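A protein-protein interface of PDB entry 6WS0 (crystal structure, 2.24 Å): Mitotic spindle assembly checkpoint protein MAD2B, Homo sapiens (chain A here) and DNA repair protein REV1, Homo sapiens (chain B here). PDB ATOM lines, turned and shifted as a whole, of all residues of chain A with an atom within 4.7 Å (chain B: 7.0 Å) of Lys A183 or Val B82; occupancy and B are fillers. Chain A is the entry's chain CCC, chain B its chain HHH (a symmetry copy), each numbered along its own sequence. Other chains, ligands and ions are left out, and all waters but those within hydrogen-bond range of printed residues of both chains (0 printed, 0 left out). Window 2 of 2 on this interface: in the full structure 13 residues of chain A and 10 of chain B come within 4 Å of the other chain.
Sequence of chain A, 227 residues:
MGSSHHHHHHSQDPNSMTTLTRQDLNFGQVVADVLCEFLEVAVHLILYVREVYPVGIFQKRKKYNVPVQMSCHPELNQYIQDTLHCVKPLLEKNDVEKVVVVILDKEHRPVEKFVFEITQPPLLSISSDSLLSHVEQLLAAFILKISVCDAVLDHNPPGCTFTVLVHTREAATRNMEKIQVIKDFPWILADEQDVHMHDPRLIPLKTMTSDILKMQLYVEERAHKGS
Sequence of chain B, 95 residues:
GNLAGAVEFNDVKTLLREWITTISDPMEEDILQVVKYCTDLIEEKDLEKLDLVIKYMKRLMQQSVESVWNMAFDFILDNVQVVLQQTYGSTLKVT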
ATOM      1  N   GLN A 180     -29.323 -16.356  23.566  1.00  0.00           N
ATOM      2  CA  GLN A 180     -28.806 -17.687  24.014  1.00  0.00           C
ATOM      3  C   GLN A 180     -27.685 -17.492  25.039  1.00  0.00           C
ATOM      4  O   GLN A 180     -26.570 -17.894  24.718  1.00  0.00           O
ATOM      5  CB  GLN A 180     -28.149 -18.503  22.881  1.00  0.00           C
ATOM      6  CG  GLN A 180     -28.990 -18.757  21.640  1.00  0.00           C
ATOM      7  CD  GLN A 180     -30.164 -19.699  21.799  1.00  0.00           C
ATOM      8  OE1 GLN A 180     -30.646 -19.971  22.902  1.00  0.00           O
ATOM      9  NE2 GLN A 180     -30.687 -20.148  20.660  1.00  0.00           N
ATOM     10  N   VAL A 181     -27.931 -16.901  26.210  1.00  0.00           N
ATOM     11  CA  VAL A 181     -26.881 -16.650  27.248  1.00  0.00           C
ATOM     12  C   VAL A 181     -27.142 -17.510  28.485  1.00  0.00           C
ATOM     13  O   VAL A 181     -26.284 -17.578  29.398  1.00  0.00           O
ATOM     14  CB  VAL A 181     -26.779 -15.171  27.654  1.00  0.00           C
ATOM     15  CG1 VAL A 181     -25.466 -14.902  28.397  1.00  0.00           C
ATOM     16  CG2 VAL A 181     -26.899 -14.227  26.484  1.00  0.00           C
ATOM     17  N   ILE A 182     -28.315 -18.090  28.591  1.00  0.00           N
ATOM     18  CA  ILE A 182     -28.613 -18.935  29.768  1.00  0.00           C
ATOM     19  C   ILE A 182     -28.457 -20.386  29.312  1.00  0.00           C
ATOM     20  O   ILE A 182     -29.245 -20.791  28.444  1.00  0.00           O
ATOM     21  CB  ILE A 182     -30.002 -18.621  30.316  1.00  0.00           C
ATOM     22  CG1 ILE A 182     -30.118 -17.172  30.791  1.00  0.00           C
ATOM     23  CG2 ILE A 182     -30.341 -19.605  31.420  1.00  0.00           C
ATOM     24  CD1 ILE A 182     -31.557 -16.755  31.170  1.00  0.00           C
ATOM     25  N   LYS A 183     -27.522 -21.159  29.879  1.00  0.00           N
ATOM     26  CA  LYS A 183     -27.410 -22.597  29.521  1.00  0.00           C
ATOM     27  C   LYS A 183     -28.525 -23.365  30.230  1.00  0.00           C
ATOM     28  O   LYS A 183     -28.920 -23.016  31.340  1.00  0.00           O
ATOM     29  CB  LYS A 183     -25.990 -23.107  29.755  1.00  0.00           C
ATOM     30  CG  LYS A 183     -24.960 -22.448  28.839  1.00  0.00           C
ATOM     31  CD  LYS A 183     -25.315 -22.396  27.333  1.00  0.00           C
ATOM     32  CE  LYS A 183     -24.797 -21.183  26.568  1.00  0.00           C
ATOM     33  NZ  LYS A 183     -25.519 -20.978  25.288  1.00  0.00           N
ATOM     34  N   ASP A 184     -29.080 -24.341  29.537  1.00  0.00           N
ATOM     35  CA  ASP A 184     -30.306 -25.045  29.976  1.00  0.00           C
ATOM     36  C   ASP A 184     -31.541 -24.197  29.616  1.00  0.00           C
ATOM     37  O   ASP A 184     -32.649 -24.693  29.901  1.00  0.00           O
ATOM     38  CB  ASP A 184     -30.241 -25.424  31.463  1.00  0.00           C
ATOM     39  CG  ASP A 184     -29.095 -26.363  31.847  1.00  0.00           C
ATOM     40  OD1 ASP A 184     -28.592 -27.084  30.958  1.00  0.00           O
ATOM     41  OD2 ASP A 184     -28.720 -26.390  33.058  1.00  0.00           O
ATOM     42  N   PHE A 185     -31.408 -22.999  29.007  1.00  0.00           N
ATOM     43  CA  PHE A 185     -32.587 -22.180  28.602  1.00  0.00           C
ATOM     44  C   PHE A 185     -32.442 -21.705  27.158  1.00  0.00           C
ATOM     45  O   PHE A 185     -32.467 -20.523  26.831  1.00  0.00           O
ATOM     46  CB  PHE A 185     -32.884 -21.027  29.563  1.00  0.00           C
ATOM     47  CG  PHE A 185     -34.345 -20.640  29.553  1.00  0.00           C
ATOM     48  CD1 PHE A 185     -35.302 -21.400  30.239  1.00  0.00           C
ATOM     49  CD2 PHE A 185     -34.771 -19.536  28.835  1.00  0.00           C
ATOM     50  CE1 PHE A 185     -36.643 -21.042  30.216  1.00  0.00           C
ATOM     51  CE2 PHE A 185     -36.102 -19.151  28.848  1.00  0.00           C
ATOM     52  CZ  PHE A 185     -37.040 -19.909  29.532  1.00  0.00           C
ATOM     53  N   PRO A 186     -32.337 -22.615  26.188  1.00  0.00           N
ATOM     54  CA  PRO A 186     -32.106 -22.173  24.822  1.00  0.00           C
ATOM     55  C   PRO A 186     -33.407 -21.662  24.198  1.00  0.00           C
ATOM     56  O   PRO A 186     -34.477 -22.072  24.583  1.00  0.00           O
ATOM     57  CB  PRO A 186     -31.670 -23.430  24.088  1.00  0.00           C
ATOM     58  CG  PRO A 186     -32.312 -24.564  24.893  1.00  0.00           C
ATOM     59  CD  PRO A 186     -32.476 -24.069  26.327  1.00  0.00           C
ATOM     60  N   LEU B  77     -24.451 -23.907  13.763  1.00  0.00           N
ATOM     61  CA  LEU B  77     -24.146 -25.013  14.677  1.00  0.00           C
ATOM     62  C   LEU B  77     -24.395 -24.566  16.125  1.00  0.00           C
ATOM     63  O   LEU B  77     -24.892 -25.417  16.929  1.00  0.00           O
ATOM     64  CB  LEU B  77     -22.697 -25.441  14.433  1.00  0.00           C
ATOM     65  CG  LEU B  77     -22.258 -26.629  15.276  1.00  0.00           C
ATOM     66  CD1 LEU B  77     -23.114 -27.853  14.939  1.00  0.00           C
ATOM     67  CD2 LEU B  77     -20.788 -26.900  15.020  1.00  0.00           C
ATOM     68  N   ASP B  78     -24.036 -23.329  16.495  1.00  0.00           N
ATOM     69  CA  ASP B  78     -24.138 -22.925  17.924  1.00  0.00           C
ATOM     70  C   ASP B  78     -25.610 -23.078  18.336  1.00  0.00           C
ATOM     71  O   ASP B  78     -25.878 -23.542  19.436  1.00  0.00           O
ATOM     72  CB  ASP B  78     -23.703 -21.479  18.195  1.00  0.00           C
ATOM     73  CG  ASP B  78     -22.203 -21.255  18.274  1.00  0.00           C
ATOM     74  OD1 ASP B  78     -21.484 -22.243  18.332  1.00  0.00           O
ATOM     75  OD2 ASP B  78     -21.775 -20.075  18.271  1.00  0.00           O
ATOM     76  N   ASN B  79     -26.530 -22.680  17.462  1.00  0.00           N
ATOM     77  CA  ASN B  79     -27.977 -22.652  17.768  1.00  0.00           C
ATOM     78  C   ASN B  79     -28.538 -24.071  17.663  1.00  0.00           C
ATOM     79  O   ASN B  79     -29.596 -24.276  18.306  1.00  0.00           O
ATOM     80  CB  ASN B  79     -28.723 -21.602  16.948  1.00  0.00           C
ATOM     81  CG  ASN B  79     -28.328 -20.236  17.450  1.00  0.00           C
ATOM     82  OD1 ASN B  79     -28.767 -19.851  18.508  1.00  0.00           O
ATOM     83  ND2 ASN B  79     -27.462 -19.523  16.744  1.00  0.00           N
ATOM     84  N   VAL B  80     -27.871 -24.991  16.946  1.00  0.00           N
ATOM     85  CA  VAL B  80     -28.317 -26.419  16.909  1.00  0.00           C
ATOM     86  C   VAL B  80     -27.823 -27.086  18.202  1.00  0.00           C
ATOM     87  O   VAL B  80     -28.619 -27.779  18.854  1.00  0.00           O
ATOM     88  CB  VAL B  80     -27.896 -27.204  15.638  1.00  0.00           C
ATOM     89  CG1 VAL B  80     -27.915 -28.724  15.851  1.00  0.00           C
ATOM     90  CG2 VAL B  80     -28.772 -26.867  14.424  1.00  0.00           C
ATOM     91  N   GLN B  81     -26.559 -26.904  18.562  1.00  0.00           N
ATOM     92  CA  GLN B  81     -26.005 -27.555  19.771  1.00  0.00           C
ATOM     93  C   GLN B  81     -26.888 -27.256  21.004  1.00  0.00           C
ATOM     94  O   GLN B  81     -27.106 -28.200  21.762  1.00  0.00           O
ATOM     95  CB  GLN B  81     -24.542 -27.167  20.001  1.00  0.00           C
ATOM     96  CG  GLN B  81     -23.610 -27.673  18.902  1.00  0.00           C
ATOM     97  CD  GLN B  81     -23.489 -29.175  18.791  1.00  0.00           C
ATOM     98  OE1 GLN B  81     -24.463 -29.931  18.833  1.00  0.00           O
ATOM     99  NE2 GLN B  81     -22.266 -29.617  18.593  1.00  0.00           N
ATOM    100  N   VAL B  82     -27.316 -26.006  21.231  1.00  0.00           N
ATOM    101  CA  VAL B  82     -28.026 -25.606  22.480  1.00  0.00           C
ATOM    102  C   VAL B  82     -29.386 -26.304  22.473  1.00  0.00           C
ATOM    103  O   VAL B  82     -29.851 -26.673  23.558  1.00  0.00           O
ATOM    104  CB  VAL B  82     -28.192 -24.086  22.630  1.00  0.00           C
ATOM    105  CG1 VAL B  82     -26.860 -23.401  22.831  1.00  0.00           C
ATOM    106  CG2 VAL B  82     -28.922 -23.460  21.447  1.00  0.00           C
ATOM    107  N   VAL B  83     -29.972 -26.539  21.296  1.00  0.00           N
ATOM    108  CA  VAL B  83     -31.240 -27.314  21.224  1.00  0.00           C
ATOM    109  C   VAL B  83     -30.934 -28.792  21.555  1.00  0.00           C
ATOM    110  O   VAL B  83     -31.637 -29.383  22.417  1.00  0.00           O
ATOM    111  CB  VAL B  83     -31.993 -27.105  19.899  1.00  0.00           C
ATOM    112  CG1 VAL B  83     -33.287 -27.897  19.880  1.00  0.00           C
ATOM    113  CG2 VAL B  83     -32.328 -25.657  19.669  1.00  0.00           C
ATOM    114  N   LEU B  84     -29.875 -29.353  20.992  1.00  0.00           N
ATOM    115  CA  LEU B  84     -29.542 -30.780  21.212  1.00  0.00           C
ATOM    116  C   LEU B  84     -29.248 -31.024  22.696  1.00  0.00           C
ATOM    117  O   LEU B  84     -29.689 -32.086  23.185  1.00  0.00           O
ATOM    118  CB  LEU B  84     -28.359 -31.211  20.325  1.00  0.00           C
ATOM    119  CG  LEU B  84     -28.682 -31.410  18.843  1.00  0.00           C
ATOM    120  CD1 LEU B  84     -27.391 -31.578  18.046  1.00  0.00           C
ATOM    121  CD2 LEU B  84     -29.610 -32.593  18.613  1.00  0.00           C
ATOM    122  N   GLN B  85     -28.508 -30.108  23.339  1.00  0.00           N
ATOM    123  CA  GLN B  85     -28.071 -30.184  24.757  1.00  0.00           C
ATOM    124  C   GLN B  85     -29.300 -30.428  25.631  1.00  0.00           C
ATOM    125  O   GLN B  85     -29.233 -31.260  26.557  1.00  0.00           O
ATOM    126  CB  GLN B  85     -27.354 -28.909  25.173  1.00  0.00           C
ATOM    127  CG  GLN B  85     -25.913 -28.819  24.700  1.00  0.00           C
ATOM    128  CD  GLN B  85     -24.959 -29.080  25.838  1.00  0.00           C
ATOM    129  OE1 GLN B  85     -25.176 -29.968  26.669  1.00  0.00           O
ATOM    130  NE2 GLN B  85     -23.898 -28.291  25.890  1.00  0.00           N
ATOM    131  N   GLN B  86     -30.400 -29.766  25.302  1.00  0.00           N
ATOM    132  CA  GLN B  86     -31.631 -29.841  26.097  1.00  0.00           C
ATOM    133  C   GLN B  86     -32.479 -31.001  25.620  1.00  0.00           C
ATOM    134  O   GLN B  86     -32.844 -31.787  26.481  1.00  0.00           O
ATOM    135  CB  GLN B  86     -32.343 -28.501  26.036  1.00  0.00           C
ATOM    136  CG  GLN B  86     -31.600 -27.488  26.872  1.00  0.00           C
ATOM    137  CD  GLN B  86     -31.402 -28.034  28.263  1.00  0.00           C
ATOM    138  OE1 GLN B  86     -30.267 -28.148  28.739  1.00  0.00           O
ATOM    139  NE2 GLN B  86     -32.516 -28.412  28.887  1.00  0.00           N
ATOM    140  N   THR B  87     -32.723 -31.170  24.314  1.00  0.00           N
ATOM    141  CA  THR B  87     -33.694 -32.188  23.832  1.00  0.00           C
ATOM    142  C   THR B  87     -33.090 -33.589  23.943  1.00  0.00           C
ATOM    143  O   THR B  87     -33.872 -34.524  24.162  1.00  0.00           O
ATOM    144  CB  THR B  87     -34.270 -31.874  22.450  1.00  0.00           C
ATOM    145  OG1 THR B  87     -33.276 -32.153  21.489  1.00  0.00           O
ATOM    146  CG2 THR B  87     -34.640 -30.431  22.258  1.00  0.00           C
ATOM    147  N   SER B  90     -27.101 -33.877  24.863  1.00  0.00           N
ATOM    148  CA  SER B  90     -25.783 -34.058  24.210  1.00  0.00           C
ATOM    149  C   SER B  90     -25.544 -33.069  23.069  1.00  0.00           C
ATOM    150  O   SER B  90     -26.458 -32.352  22.596  1.00  0.00           O
ATOM    151  CB  SER B  90     -25.622 -35.511  23.788  1.00  0.00           C
ATOM    152  OG  SER B  90     -26.610 -35.891  22.830  1.00  0.00           O
ATOM    153  N   THR B  91     -24.324 -33.113  22.589  1.00  0.00           N
ATOM    154  CA  THR B  91     -23.764 -32.190  21.601  1.00  0.00           C
ATOM    155  C   THR B  91     -23.445 -33.025  20.352  1.00  0.00           C
ATOM    156  O   THR B  91     -22.766 -34.120  20.496  1.00  0.00           O
ATOM    157  CB  THR B  91     -22.590 -31.472  22.290  1.00  0.00           C
ATOM    158  OG1 THR B  91     -23.234 -30.586  23.200  1.00  0.00           O
ATOM    159  CG2 THR B  91     -21.674 -30.701  21.362  1.00  0.00           C
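Hydrophobic or aromatic side chains of chain B that line the printed part of chain A: Val B82.
Along chain A the printed residues that touch a printed residue of chain B span positions 180 to 186.
Val B82 touches just these residues of chain A: Gln A180 (3.8 Å), Lys A183 (3.7 Å) and Pro A186 (3.5 Å).
Of the printed residues of chain A, Gln B86 touches Asp A184 and Pro A186.
Printed residues of chain B within 4 Å of Asp A184: Gln B86 (3.0 Å).
Of the printed residues of chain A, Asn B79 touches Gln A180 (2.9 Å).
Of the printed residues of chain B, Pro A186 touches Val B82 (3.5 Å) and Gln B86 (3.6 Å).
Thr B87 touches none of the printed residues of chain A.
The nearest printed residue of chain B that does not touch Gln A180 is Val B83 (5.8 Å).
The backbone carbonyl oxygen (O) of Gln A180 sits at hydrogen-bond distance from the side-chain amino group (NZ) of Lys A183 (3.3 Å).
Gln A180 touches Val B82 (NE2 to CG2, 3.8 Å).
Lys A183 touches Val B82 (NZ to CG1, 3.7 Å).
Pro A186 touches Val B82.
CD of Pro A186 touches CG of Gln B86, 3.6 Å away.
The side-chain amide nitrogen (NE2) of Gln A180 sits at hydrogen-bond distance from the side-chain amide oxygen (OD1) of Asn B79 (2.9 Å).
The side-chain amide oxygen (OE1) of Gln B86 sits close to the side-chain carboxylate (OD1) of Asp A184 (3.0 Å).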
